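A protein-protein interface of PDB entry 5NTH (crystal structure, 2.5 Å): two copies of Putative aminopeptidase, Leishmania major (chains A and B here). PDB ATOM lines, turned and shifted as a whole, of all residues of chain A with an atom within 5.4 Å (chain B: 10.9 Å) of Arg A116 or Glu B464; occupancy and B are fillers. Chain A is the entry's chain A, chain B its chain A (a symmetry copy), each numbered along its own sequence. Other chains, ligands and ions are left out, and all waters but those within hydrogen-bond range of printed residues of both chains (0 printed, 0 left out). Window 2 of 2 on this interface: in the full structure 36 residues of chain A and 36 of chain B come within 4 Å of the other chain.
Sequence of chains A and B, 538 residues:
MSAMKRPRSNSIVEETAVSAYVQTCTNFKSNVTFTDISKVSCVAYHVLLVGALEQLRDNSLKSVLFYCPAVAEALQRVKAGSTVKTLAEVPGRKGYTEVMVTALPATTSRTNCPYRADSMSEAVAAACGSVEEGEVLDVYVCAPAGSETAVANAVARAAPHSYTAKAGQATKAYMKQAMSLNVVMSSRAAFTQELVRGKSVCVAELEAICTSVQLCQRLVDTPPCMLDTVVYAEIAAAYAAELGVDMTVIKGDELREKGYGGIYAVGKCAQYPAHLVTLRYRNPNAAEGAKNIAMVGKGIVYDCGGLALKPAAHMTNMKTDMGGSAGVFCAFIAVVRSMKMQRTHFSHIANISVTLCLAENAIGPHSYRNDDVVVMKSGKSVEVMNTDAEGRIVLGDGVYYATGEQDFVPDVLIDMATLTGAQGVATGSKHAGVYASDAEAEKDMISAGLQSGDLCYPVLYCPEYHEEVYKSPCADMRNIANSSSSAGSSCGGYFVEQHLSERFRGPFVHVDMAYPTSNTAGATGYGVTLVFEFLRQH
Among the printed residues, merely in contact across the chains: Arg A116 with Glu B464 (3.6 Å), Asn A112 with Tyr B465 (3.8 Å), Ser A109 with Pro B463 (3.8 Å), Thr A108 with Glu B464 (3.9 Å) and Ser A109 with Tyr B461 (3.997 Å).
Of the 23 printed residues of chain B, 5 touch a printed residue of chain A. Printed residues of chain B that touch a printed residue of chain A: Tyr B461, Cys B462, Pro B463, Glu B464 and Tyr B465. Hydrophobic or aromatic side chains of chain B that line the printed part of chain A: Pro B463 and Tyr B465. Of the 14 printed residues of chain A, 5 touch a printed residue of chain B. Among the printed residues, 9 pairs touch across the chains. Among the printed residues, no Asp or Glu carboxylate lies within 4 Å of a Lys or Arg side-chain nitrogen of the other chain.
No residue of chain B comes within 4 Å of Pro A105. Of chain B, only Glu B464 comes within 4 Å of Thr A108. Printed residues of chain B within 4 Å of Asn A112: Glu B464 (2.8 Å) and Tyr B465 (3.8 Å). Cys A113 touches none of the printed residues of chain B. No residue of chain B comes within 4 Å of Pro A114. Of chain B, only Glu B464 (3.6 Å) comes within 4 Å of Arg A116. Ala A117 touches none of the printed residues of chain B. Of chain B, only Tyr B465 comes within 4 Å of Asp A118. No residue of chain B comes within 4 Å of Ser A119. No residue of chain B comes within 4 Å of Met A120. Of the printed residues of chain A, Cys B462 touches Ser A109. Glu B464 touches four residues of chain A. Of the printed residues of chain A, Tyr B465 touches Asn A112 and Asp A118. Lys B471 touches none of the printed residues of chain A. Tyr B494 touches none of the printed residues of chain A. The nearest printed residue of chain A that does not touch Tyr B461 is Asn A112 (5.8 Å).
The side-chain amide nitrogen (ND2) of Asn A112 sits at hydrogen-bond distance from the side-chain carboxylate (OD2) of Asp A118 (3.2 Å). The backbone NH of Cys B462 lies within hydrogen-bond range of a ring nitrogen (NE2) of His B466, at 3.2 Å. The guanidinium group (NH1) of Arg A116 lies within hydrogen-bond range of the side-chain hydroxyl (OG) of Ser A119, at 3.3 Å.
No position is printed for both chains.
OD2 of Asp A118 lies close to OH of Tyr B465. The side-chain carboxylate (OE1) of Glu B464 is in hydrogen-bond range of the side-chain hydroxyl (OG) of Ser A109, at 2.6 Å. The side-chain amide nitrogen (ND2) of Asn A112 is in hydrogen-bond range of the side-chain carboxylate (OE2) of Glu B464 (2.8 Å). SG of Cys B462 lies close to OG of Ser A109, at 3.8 Å.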
ATOM      1  N   LEU A 104     -14.326  26.737 -19.233  1.00  0.00           N
ATOM      2  CA  LEU A 104     -15.126  25.577 -19.001  1.00  0.00           C
ATOM      3  C   LEU A 104     -14.952  24.667 -20.194  1.00  0.00           C
ATOM      4  O   LEU A 104     -14.453  25.097 -21.234  1.00  0.00           O
ATOM      5  CB  LEU A 104     -16.589  25.937 -18.827  1.00  0.00           C
ATOM      6  CG  LEU A 104     -16.914  26.933 -17.692  1.00  0.00           C
ATOM      7  CD1 LEU A 104     -18.346  27.467 -17.822  1.00  0.00           C
ATOM      8  CD2 LEU A 104     -16.637  26.373 -16.293  1.00  0.00           C
ATOM      9  N   PRO A 105     -15.336  23.386 -20.038  1.00  0.00           N
ATOM     10  CA  PRO A 105     -15.177  22.438 -21.139  1.00  0.00           C
ATOM     11  C   PRO A 105     -16.102  22.693 -22.321  1.00  0.00           C
ATOM     12  O   PRO A 105     -17.221  23.257 -22.179  1.00  0.00           O
ATOM     13  CB  PRO A 105     -15.494  21.084 -20.486  1.00  0.00           C
ATOM     14  CG  PRO A 105     -15.255  21.303 -19.021  1.00  0.00           C
ATOM     15  CD  PRO A 105     -15.779  22.685 -18.810  1.00  0.00           C
ATOM     16  N   THR A 107     -17.676  20.515 -24.445  1.00  0.00           N
ATOM     17  CA  THR A 107     -18.817  19.639 -24.730  1.00  0.00           C
ATOM     18  C   THR A 107     -19.450  19.104 -23.439  1.00  0.00           C
ATOM     19  O   THR A 107     -18.769  18.690 -22.507  1.00  0.00           O
ATOM     20  CB  THR A 107     -18.399  18.465 -25.671  1.00  0.00           C
ATOM     21  OG1 THR A 107     -17.386  17.669 -25.047  1.00  0.00           O
ATOM     22  CG2 THR A 107     -17.809  18.987 -26.991  1.00  0.00           C
ATOM     23  N   THR A 108     -20.773  19.118 -23.415  1.00  0.00           N
ATOM     24  CA  THR A 108     -21.559  18.647 -22.283  1.00  0.00           C
ATOM     25  C   THR A 108     -22.599  17.637 -22.777  1.00  0.00           C
ATOM     26  O   THR A 108     -23.140  17.789 -23.851  1.00  0.00           O
ATOM     27  CB  THR A 108     -22.187  19.859 -21.558  1.00  0.00           C
ATOM     28  OG1 THR A 108     -21.189  20.430 -20.700  1.00  0.00           O
ATOM     29  CG2 THR A 108     -23.402  19.486 -20.719  1.00  0.00           C
ATOM     30  N   SER A 109     -22.889  16.616 -21.985  1.00  0.00           N
ATOM     31  CA  SER A 109     -23.892  15.642 -22.380  1.00  0.00           C
ATOM     32  C   SER A 109     -25.240  15.863 -21.692  1.00  0.00           C
ATOM     33  O   SER A 109     -25.380  16.663 -20.748  1.00  0.00           O
ATOM     34  CB  SER A 109     -23.364  14.248 -22.154  1.00  0.00           C
ATOM     35  OG  SER A 109     -22.895  14.169 -20.842  1.00  0.00           O
ATOM     36  N   ASN A 112     -25.816  16.015 -17.768  1.00  0.00           N
ATOM     37  CA  ASN A 112     -25.020  16.925 -16.989  1.00  0.00           C
ATOM     38  C   ASN A 112     -25.599  18.317 -17.082  1.00  0.00           C
ATOM     39  O   ASN A 112     -26.353  18.655 -17.992  1.00  0.00           O
ATOM     40  CB  ASN A 112     -23.564  16.927 -17.489  1.00  0.00           C
ATOM     41  CG  ASN A 112     -22.571  17.556 -16.497  1.00  0.00           C
ATOM     42  OD1 ASN A 112     -22.943  18.050 -15.416  1.00  0.00           O
ATOM     43  ND2 ASN A 112     -21.294  17.540 -16.870  1.00  0.00           N
ATOM     44  N   CYS A 113     -25.221  19.115 -16.106  1.00  0.00           N
ATOM     45  CA  CYS A 113     -25.686  20.452 -15.982  1.00  0.00           C
ATOM     46  C   CYS A 113     -25.075  21.276 -17.094  1.00  0.00           C
ATOM     47  O   CYS A 113     -23.855  21.365 -17.191  1.00  0.00           O
ATOM     48  CB  CYS A 113     -25.262  20.974 -14.621  1.00  0.00           C
ATOM     49  SG  CYS A 113     -25.285  22.754 -14.527  1.00  0.00           S
ATOM     50  N   PRO A 114     -25.916  21.913 -17.921  1.00  0.00           N
ATOM     51  CA  PRO A 114     -25.444  22.670 -19.115  1.00  0.00           C
ATOM     52  C   PRO A 114     -24.586  23.912 -18.815  1.00  0.00           C
ATOM     53  O   PRO A 114     -23.874  24.407 -19.689  1.00  0.00           O
ATOM     54  CB  PRO A 114     -26.740  23.106 -19.774  1.00  0.00           C
ATOM     55  CG  PRO A 114     -27.618  23.333 -18.599  1.00  0.00           C
ATOM     56  CD  PRO A 114     -27.323  22.214 -17.634  1.00  0.00           C
ATOM     57  N   TYR A 115     -24.674  24.402 -17.583  1.00  0.00           N
ATOM     58  CA  TYR A 115     -23.816  25.483 -17.105  1.00  0.00           C
ATOM     59  C   TYR A 115     -22.442  24.985 -16.644  1.00  0.00           C
ATOM     60  O   TYR A 115     -21.580  25.795 -16.374  1.00  0.00           O
ATOM     61  CB  TYR A 115     -24.490  26.202 -15.932  1.00  0.00           C
ATOM     62  CG  TYR A 115     -25.957  26.496 -16.149  1.00  0.00           C
ATOM     63  CD1 TYR A 115     -26.411  27.050 -17.362  1.00  0.00           C
ATOM     64  CD2 TYR A 115     -26.893  26.215 -15.162  1.00  0.00           C
ATOM     65  CE1 TYR A 115     -27.753  27.312 -17.578  1.00  0.00           C
ATOM     66  CE2 TYR A 115     -28.250  26.461 -15.372  1.00  0.00           C
ATOM     67  CZ  TYR A 115     -28.683  27.023 -16.577  1.00  0.00           C
ATOM     68  OH  TYR A 115     -30.030  27.273 -16.780  1.00  0.00           O
ATOM     69  N   ARG A 116     -22.258  23.666 -16.543  1.00  0.00           N
ATOM     70  CA  ARG A 116     -21.022  23.025 -16.089  1.00  0.00           C
ATOM     71  C   ARG A 116     -20.571  23.494 -14.747  1.00  0.00           C
ATOM     72  O   ARG A 116     -19.441  23.891 -14.580  1.00  0.00           O
ATOM     73  CB  ARG A 116     -19.891  23.128 -17.122  1.00  0.00           C
ATOM     74  CG  ARG A 116     -20.082  22.198 -18.322  1.00  0.00           C
ATOM     75  CD  ARG A 116     -20.149  20.728 -17.891  1.00  0.00           C
ATOM     76  NE  ARG A 116     -19.244  19.946 -18.712  1.00  0.00           N
ATOM     77  CZ  ARG A 116     -18.167  19.306 -18.271  1.00  0.00           C
ATOM     78  NH1 ARG A 116     -17.843  19.297 -16.982  1.00  0.00           N
ATOM     79  NH2 ARG A 116     -17.395  18.663 -19.146  1.00  0.00           N
ATOM     80  N   ALA A 117     -21.474  23.390 -13.780  1.00  0.00           N
ATOM     81  CA  ALA A 117     -21.198  23.698 -12.374  1.00  0.00           C
ATOM     82  C   ALA A 117     -20.081  22.868 -11.738  1.00  0.00           C
ATOM     83  O   ALA A 117     -19.525  23.269 -10.722  1.00  0.00           O
ATOM     84  CB  ALA A 117     -22.470  23.543 -11.564  1.00  0.00           C
ATOM     85  N   ASP A 118     -19.785  21.716 -12.310  1.00  0.00           N
ATOM     86  CA  ASP A 118     -18.671  20.901 -11.844  1.00  0.00           C
ATOM     87  C   ASP A 118     -17.318  21.552 -12.095  1.00  0.00           C
ATOM     88  O   ASP A 118     -16.463  21.586 -11.225  1.00  0.00           O
ATOM     89  CB  ASP A 118     -18.693  19.465 -12.437  1.00  0.00           C
ATOM     90  CG  ASP A 118     -19.077  19.413 -13.914  1.00  0.00           C
ATOM     91  OD1 ASP A 118     -18.980  20.438 -14.629  1.00  0.00           O
ATOM     92  OD2 ASP A 118     -19.507  18.335 -14.363  1.00  0.00           O
ATOM     93  N   SER A 119     -17.130  22.044 -13.302  1.00  0.00           N
ATOM     94  CA  SER A 119     -15.904  22.719 -13.657  1.00  0.00           C
ATOM     95  C   SER A 119     -15.747  24.041 -12.903  1.00  0.00           C
ATOM     96  O   SER A 119     -14.649  24.425 -12.526  1.00  0.00           O
ATOM     97  CB  SER A 119     -15.881  22.924 -15.159  1.00  0.00           C
ATOM     98  OG  SER A 119     -15.886  21.657 -15.794  1.00  0.00           O
ATOM     99  N   MET A 120     -16.863  24.711 -12.658  1.00  0.00           N
ATOM    100  CA  MET A 120     -16.870  25.952 -11.880  1.00  0.00           C
ATOM    101  C   MET A 120     -16.343  25.691 -10.491  1.00  0.00           C
ATOM    102  O   MET A 120     -15.514  26.426 -10.003  1.00  0.00           O
ATOM    103  CB  MET A 120     -18.280  26.531 -11.754  1.00  0.00           C
ATOM    104  CG  MET A 120     -18.840  27.134 -13.023  1.00  0.00           C
ATOM    105  SD  MET A 120     -20.415  28.019 -12.778  1.00  0.00           S
ATOM    106  CE  MET A 120     -20.605  28.658 -14.449  1.00  0.00           C
ATOM    107  N   TYR B 435     -26.877   1.878 -22.769  1.00  0.00           N
ATOM    108  CA  TYR B 435     -26.014   3.040 -22.754  1.00  0.00           C
ATOM    109  C   TYR B 435     -26.124   3.607 -24.140  1.00  0.00           C
ATOM    110  O   TYR B 435     -25.620   3.021 -25.097  1.00  0.00           O
ATOM    111  CB  TYR B 435     -24.575   2.653 -22.465  1.00  0.00           C
ATOM    112  CG  TYR B 435     -23.564   3.775 -22.658  1.00  0.00           C
ATOM    113  CD1 TYR B 435     -23.310   4.711 -21.648  1.00  0.00           C
ATOM    114  CD2 TYR B 435     -22.832   3.861 -23.829  1.00  0.00           C
ATOM    115  CE1 TYR B 435     -22.374   5.693 -21.816  1.00  0.00           C
ATOM    116  CE2 TYR B 435     -21.891   4.847 -24.012  1.00  0.00           C
ATOM    117  CZ  TYR B 435     -21.662   5.763 -23.010  1.00  0.00           C
ATOM    118  OH  TYR B 435     -20.715   6.735 -23.243  1.00  0.00           O
ATOM    119  N   ALA B 436     -26.782   4.749 -24.241  1.00  0.00           N
ATOM    120  CA  ALA B 436     -27.275   5.211 -25.519  1.00  0.00           C
ATOM    121  C   ALA B 436     -26.941   6.655 -25.747  1.00  0.00           C
ATOM    122  O   ALA B 436     -27.289   7.484 -24.918  1.00  0.00           O
ATOM    123  CB  ALA B 436     -28.779   5.025 -25.554  1.00  0.00           C
ATOM    124  N   SER B 437     -26.341   6.946 -26.901  1.00  0.00           N
ATOM    125  CA  SER B 437     -25.944   8.328 -27.277  1.00  0.00           C
ATOM    126  C   SER B 437     -27.059   9.219 -27.813  1.00  0.00           C
ATOM    127  O   SER B 437     -26.778  10.305 -28.248  1.00  0.00           O
ATOM    128  CB  SER B 437     -24.890   8.279 -28.378  1.00  0.00           C
ATOM    129  OG  SER B 437     -25.486   7.722 -29.541  1.00  0.00           O
ATOM    130  N   LEU B 460     -26.561   5.554 -17.052  1.00  0.00           N
ATOM    131  CA  LEU B 460     -25.945   6.856 -17.180  1.00  0.00           C
ATOM    132  C   LEU B 460     -25.151   7.011 -18.477  1.00  0.00           C
ATOM    133  O   LEU B 460     -24.283   6.221 -18.742  1.00  0.00           O
ATOM    134  CB  LEU B 460     -25.043   7.090 -15.978  1.00  0.00           C
ATOM    135  CG  LEU B 460     -24.412   8.478 -15.886  1.00  0.00           C
ATOM    136  CD1 LEU B 460     -25.479   9.570 -15.775  1.00  0.00           C
ATOM    137  CD2 LEU B 460     -23.430   8.544 -14.731  1.00  0.00           C
ATOM    138  N   TYR B 461     -25.500   7.998 -19.306  1.00  0.00           N
ATOM    139  CA  TYR B 461     -24.670   8.375 -20.461  1.00  0.00           C
ATOM    140  C   TYR B 461     -24.028   9.724 -20.115  1.00  0.00           C
ATOM    141  O   TYR B 461     -24.735  10.735 -19.950  1.00  0.00           O
ATOM    142  CB  TYR B 461     -25.484   8.475 -21.749  1.00  0.00           C
ATOM    143  CG  TYR B 461     -24.665   8.839 -22.983  1.00  0.00           C
ATOM    144  CD1 TYR B 461     -24.043   7.865 -23.740  1.00  0.00           C
ATOM    145  CD2 TYR B 461     -24.531  10.173 -23.394  1.00  0.00           C
ATOM    146  CE1 TYR B 461     -23.303   8.199 -24.859  1.00  0.00           C
ATOM    147  CE2 TYR B 461     -23.771  10.522 -24.501  1.00  0.00           C
ATOM    148  CZ  TYR B 461     -23.171   9.536 -25.216  1.00  0.00           C
ATOM    149  OH  TYR B 461     -22.461   9.882 -26.287  1.00  0.00           O
ATOM    150  N   CYS B 462     -22.702   9.733 -19.992  1.00  0.00           N
ATOM    151  CA  CYS B 462     -21.988  10.912 -19.539  1.00  0.00           C
ATOM    152  C   CYS B 462     -20.514  10.804 -19.877  1.00  0.00           C
ATOM    153  O   CYS B 462     -19.697  10.720 -18.981  1.00  0.00           O
ATOM    154  CB  CYS B 462     -22.190  11.113 -18.034  1.00  0.00           C
ATOM    155  SG  CYS B 462     -21.742  12.776 -17.516  1.00  0.00           S
ATOM    156  N   PRO B 463     -20.172  10.806 -21.180  1.00  0.00           N
ATOM    157  CA  PRO B 463     -18.794  10.652 -21.636  1.00  0.00           C
ATOM    158  C   PRO B 463     -17.799  11.610 -20.989  1.00  0.00           C
ATOM    159  O   PRO B 463     -16.653  11.238 -20.806  1.00  0.00           O
ATOM    160  CB  PRO B 463     -18.878  10.957 -23.138  1.00  0.00           C
ATOM    161  CG  PRO B 463     -20.277  10.677 -23.508  1.00  0.00           C
ATOM    162  CD  PRO B 463     -21.062  11.122 -22.307  1.00  0.00           C
ATOM    163  N   GLU B 464     -18.210  12.833 -20.662  1.00  0.00           N
ATOM    164  CA  GLU B 464     -17.274  13.746 -19.983  1.00  0.00           C
ATOM    165  C   GLU B 464     -16.807  13.198 -18.640  1.00  0.00           C
ATOM    166  O   GLU B 464     -15.650  13.360 -18.287  1.00  0.00           O
ATOM    167  CB  GLU B 464     -17.806  15.162 -19.808  1.00  0.00           C
ATOM    168  CG  GLU B 464     -19.038  15.347 -18.915  1.00  0.00           C
ATOM    169  CD  GLU B 464     -20.322  15.458 -19.709  1.00  0.00           C
ATOM    170  OE1 GLU B 464     -20.415  14.801 -20.766  1.00  0.00           O
ATOM    171  OE2 GLU B 464     -21.231  16.206 -19.290  1.00  0.00           O
ATOM    172  N   TYR B 465     -17.690  12.528 -17.922  1.00  0.00           N
ATOM    173  CA  TYR B 465     -17.331  11.913 -16.654  1.00  0.00           C
ATOM    174  C   TYR B 465     -16.594  10.605 -16.854  1.00  0.00           C
ATOM    175  O   TYR B 465     -15.656  10.328 -16.095  1.00  0.00           O
ATOM    176  CB  TYR B 465     -18.581  11.765 -15.773  1.00  0.00           C
ATOM    177  CG  TYR B 465     -19.025  13.059 -15.084  1.00  0.00           C
ATOM    178  CD1 TYR B 465     -18.389  14.311 -15.314  1.00  0.00           C
ATOM    179  CD2 TYR B 465     -20.081  13.040 -14.200  1.00  0.00           C
ATOM    180  CE1 TYR B 465     -18.796  15.473 -14.642  1.00  0.00           C
ATOM    181  CE2 TYR B 465     -20.514  14.202 -13.552  1.00  0.00           C
ATOM    182  CZ  TYR B 465     -19.868  15.417 -13.758  1.00  0.00           C
ATOM    183  OH  TYR B 465     -20.344  16.508 -13.068  1.00  0.00           O
ATOM    184  N   HIS B 466     -16.957   9.830 -17.885  1.00  0.00           N
ATOM    185  CA  HIS B 466     -16.242   8.563 -18.183  1.00  0.00           C
ATOM    186  C   HIS B 466     -14.834   8.831 -18.716  1.00  0.00           C
ATOM    187  O   HIS B 466     -13.897   8.126 -18.360  1.00  0.00           O
ATOM    188  CB  HIS B 466     -16.990   7.629 -19.158  1.00  0.00           C
ATOM    189  CG  HIS B 466     -18.455   7.524 -18.888  1.00  0.00           C
ATOM    190  ND1 HIS B 466     -18.970   7.416 -17.614  1.00  0.00           N
ATOM    191  CD2 HIS B 466     -19.520   7.560 -19.718  1.00  0.00           C
ATOM    192  CE1 HIS B 466     -20.286   7.393 -17.671  1.00  0.00           C
ATOM    193  NE2 HIS B 466     -20.645   7.484 -18.934  1.00  0.00           N
ATOM    194  N   GLU B 467     -14.680   9.851 -19.552  1.00  0.00           N
ATOM    195  CA  GLU B 467     -13.389  10.182 -20.114  1.00  0.00           C
ATOM    196  C   GLU B 467     -12.370  10.321 -19.019  1.00  0.00           C
ATOM    197  O   GLU B 467     -11.229   9.893 -19.188  1.00  0.00           O
ATOM    198  CB  GLU B 467     -13.450  11.476 -20.913  1.00  0.00           C
ATOM    199  CG  GLU B 467     -12.106  11.834 -21.535  1.00  0.00           C
ATOM    200  CD  GLU B 467     -12.167  13.033 -22.476  1.00  0.00           C
ATOM    201  OE1 GLU B 467     -12.811  14.059 -22.119  1.00  0.00           O
ATOM    202  OE2 GLU B 467     -11.546  12.958 -23.576  1.00  0.00           O
ATOM    203  N   GLU B 468     -12.790  10.913 -17.903  1.00  0.00           N
ATOM    204  CA  GLU B 468     -11.856  11.274 -16.848  1.00  0.00           C
ATOM    205  C   GLU B 468     -11.518  10.158 -15.876  1.00  0.00           C
ATOM    206  O   GLU B 468     -10.732  10.384 -14.987  1.00  0.00           O
ATOM    207  CB  GLU B 468     -12.293  12.553 -16.089  1.00  0.00           C
ATOM    208  CG  GLU B 468     -13.406  12.406 -15.035  1.00  0.00           C
ATOM    209  CD  GLU B 468     -13.632  13.681 -14.190  1.00  0.00           C
ATOM    210  OE1 GLU B 468     -12.657  14.099 -13.511  1.00  0.00           O
ATOM    211  OE2 GLU B 468     -14.772  14.252 -14.186  1.00  0.00           O
ATOM    212  N   VAL B 469     -12.084   8.971 -16.024  1.00  0.00           N
ATOM    213  CA  VAL B 469     -11.619   7.817 -15.247  1.00  0.00           C
ATOM    214  C   VAL B 469     -10.846   6.778 -16.081  1.00  0.00           C
ATOM    215  O   VAL B 469     -10.398   5.784 -15.551  1.00  0.00           O
ATOM    216  CB  VAL B 469     -12.752   7.153 -14.425  1.00  0.00           C
ATOM    217  CG1 VAL B 469     -13.358   8.154 -13.454  1.00  0.00           C
ATOM    218  CG2 VAL B 469     -13.834   6.521 -15.296  1.00  0.00           C
ATOM    219  N   TYR B 470     -10.662   7.052 -17.366  1.00  0.00           N
ATOM    220  CA  TYR B 470      -9.918   6.205 -18.311  1.00  0.00           C
ATOM    221  C   TYR B 470      -8.570   6.792 -18.767  1.00  0.00           C
ATOM    222  O   TYR B 470      -7.929   6.238 -19.699  1.00  0.00           O
ATOM    223  CB  TYR B 470     -10.760   6.025 -19.578  1.00  0.00           C
ATOM    224  CG  TYR B 470     -11.674   4.862 -19.585  1.00  0.00           C
ATOM    225  CD1 TYR B 470     -11.183   3.578 -19.628  1.00  0.00           C
ATOM    226  CD2 TYR B 470     -13.032   5.045 -19.628  1.00  0.00           C
ATOM    227  CE1 TYR B 470     -12.032   2.490 -19.646  1.00  0.00           C
ATOM    228  CE2 TYR B 470     -13.894   3.967 -19.667  1.00  0.00           C
ATOM    229  CZ  TYR B 470     -13.377   2.687 -19.659  1.00  0.00           C
ATOM    230  OH  TYR B 470     -14.208   1.606 -19.712  1.00  0.00           O
ATOM    231  N   LYS B 471      -8.172   7.922 -18.167  1.00  0.00           N
ATOM    232  CA  LYS B 471      -6.907   8.564 -18.494  1.00  0.00           C
ATOM    233  C   LYS B 471      -5.746   7.586 -18.236  1.00  0.00           C
ATOM    234  O   LYS B 471      -5.700   6.944 -17.186  1.00  0.00           O
ATOM    235  CB  LYS B 471      -6.720   9.812 -17.651  1.00  0.00           C
ATOM    236  CG  LYS B 471      -7.669  10.963 -17.959  1.00  0.00           C
ATOM    237  CD  LYS B 471      -7.406  12.164 -17.025  1.00  0.00           C
ATOM    238  CE  LYS B 471      -7.486  13.544 -17.715  1.00  0.00           C
ATOM    239  NZ  LYS B 471      -8.844  13.858 -18.278  1.00  0.00           N
ATOM    240  N   SER B 486     -17.473   3.854 -10.426  1.00  0.00           N
ATOM    241  CA  SER B 486     -17.520   4.844 -11.477  1.00  0.00           C
ATOM    242  C   SER B 486     -18.408   4.190 -12.499  1.00  0.00           C
ATOM    243  O   SER B 486     -17.915   3.740 -13.524  1.00  0.00           O
ATOM    244  CB  SER B 486     -16.120   5.113 -12.060  1.00  0.00           C
ATOM    245  N   ALA B 487     -19.690   4.040 -12.166  1.00  0.00           N
ATOM    246  CA  ALA B 487     -20.735   3.762 -13.158  1.00  0.00           C
ATOM    247  C   ALA B 487     -20.261   2.743 -14.193  1.00  0.00           C
ATOM    248  O   ALA B 487     -20.072   3.063 -15.374  1.00  0.00           O
ATOM    249  CB  ALA B 487     -21.165   5.062 -13.829  1.00  0.00           C
ATOM    250  N   SER B 490     -21.835   1.872 -17.798  1.00  0.00           N
ATOM    251  CA  SER B 490     -21.675   2.964 -18.761  1.00  0.00           C
ATOM    252  C   SER B 490     -20.241   3.042 -19.252  1.00  0.00           C
ATOM    253  O   SER B 490     -19.997   3.236 -20.439  1.00  0.00           O
ATOM    254  CB  SER B 490     -22.043   4.298 -18.165  1.00  0.00           C
ATOM    255  OG  SER B 490     -23.090   4.180 -17.222  1.00  0.00           O
ATOM    256  N   CYS B 491     -19.292   2.893 -18.335  1.00  0.00           N
ATOM    257  CA  CYS B 491     -17.881   2.940 -18.694  1.00  0.00           C
ATOM    258  C   CYS B 491     -17.562   1.869 -19.763  1.00  0.00           C
ATOM    259  O   CYS B 491     -16.763   2.089 -20.674  1.00  0.00           O
ATOM    260  CB  CYS B 491     -16.979   2.837 -17.416  1.00  0.00           C
ATOM    261  SG  CYS B 491     -16.972   4.326 -16.325  1.00  0.00           S
ATOM    262  N   TYR B 494     -18.932   3.335 -23.029  1.00  0.00           N
ATOM    263  CA  TYR B 494     -18.075   4.465 -23.431  1.00  0.00           C
ATOM    264  C   TYR B 494     -16.778   4.011 -24.082  1.00  0.00           C
ATOM    265  O   TYR B 494     -16.322   4.593 -25.052  1.00  0.00           O
ATOM    266  CB  TYR B 494     -17.760   5.342 -22.210  1.00  0.00           C
ATOM    267  CG  TYR B 494     -16.701   6.390 -22.456  1.00  0.00           C
ATOM    268  CD1 TYR B 494     -17.019   7.618 -23.047  1.00  0.00           C
ATOM    269  CD2 TYR B 494     -15.366   6.146 -22.102  1.00  0.00           C
ATOM    270  CE1 TYR B 494     -16.037   8.565 -23.285  1.00  0.00           C
ATOM    271  CE2 TYR B 494     -14.374   7.080 -22.331  1.00  0.00           C
ATOM    272  CZ  TYR B 494     -14.711   8.286 -22.918  1.00  0.00           C
ATOM    273  OH  TYR B 494     -13.720   9.204 -23.152  1.00  0.00           O
ATOM    274  N   PHE B 495     -16.193   2.959 -23.549  1.00  0.00           N
ATOM    275  CA  PHE B 495     -14.991   2.445 -24.135  1.00  0.00           C
ATOM    276  C   PHE B 495     -15.292   2.122 -25.572  1.00  0.00           C
ATOM    277  O   PHE B 495     -14.618   2.594 -26.436  1.00  0.00           O
ATOM    278  CB  PHE B 495     -14.480   1.197 -23.428  1.00  0.00           C
ATOM    279  CG  PHE B 495     -13.219   0.682 -24.022  1.00  0.00           C
ATOM    280  CD1 PHE B 495     -13.246  -0.153 -25.137  1.00  0.00           C
ATOM    281  CD2 PHE B 495     -11.991   1.098 -23.530  1.00  0.00           C
ATOM    282  CE1 PHE B 495     -12.060  -0.608 -25.724  1.00  0.00           C
ATOM    283  CE2 PHE B 495     -10.812   0.642 -24.107  1.00  0.00           C
ATOM    284  CZ  PHE B 495     -10.850  -0.209 -25.213  1.00  0.00           C
ATOM    285  N   GLU B 497     -17.815   3.030 -27.480  1.00  0.00           N
ATOM    286  CA  GLU B 497     -18.192   4.195 -28.247  1.00  0.00           C
ATOM    287  C   GLU B 497     -16.991   4.911 -28.886  1.00  0.00           C
ATOM    288  O   GLU B 497     -17.093   5.421 -30.006  1.00  0.00           O
ATOM    289  CB  GLU B 497     -18.936   5.175 -27.373  1.00  0.00           C
ATOM    290  CG  GLU B 497     -19.683   6.228 -28.153  1.00  0.00           C
ATOM    291  CD  GLU B 497     -20.415   7.181 -27.243  1.00  0.00           C
ATOM    292  OE1 GLU B 497     -20.126   7.172 -26.028  1.00  0.00           O
ATOM    293  OE2 GLU B 497     -21.284   7.946 -27.741  1.00  0.00           O
ATOM    294  N   GLN B 498     -15.844   4.930 -28.215  1.00  0.00           N
ATOM    295  CA  GLN B 498     -14.731   5.703 -28.746  1.00  0.00           C
ATOM    296  C   GLN B 498     -14.169   5.144 -30.026  1.00  0.00           C
ATOM    297  O   GLN B 498     -13.412   5.830 -30.677  1.00  0.00           O
ATOM    298  CB  GLN B 498     -13.601   5.811 -27.740  1.00  0.00           C
ATOM    299  CG  GLN B 498     -13.971   6.350 -26.379  1.00  0.00           C
ATOM    300  CD  GLN B 498     -14.938   7.515 -26.451  1.00  0.00           C
ATOM    301  OE1 GLN B 498     -16.138   7.344 -26.212  1.00  0.00           O
ATOM    302  NE2 GLN B 498     -14.442   8.688 -26.804  1.00  0.00           N
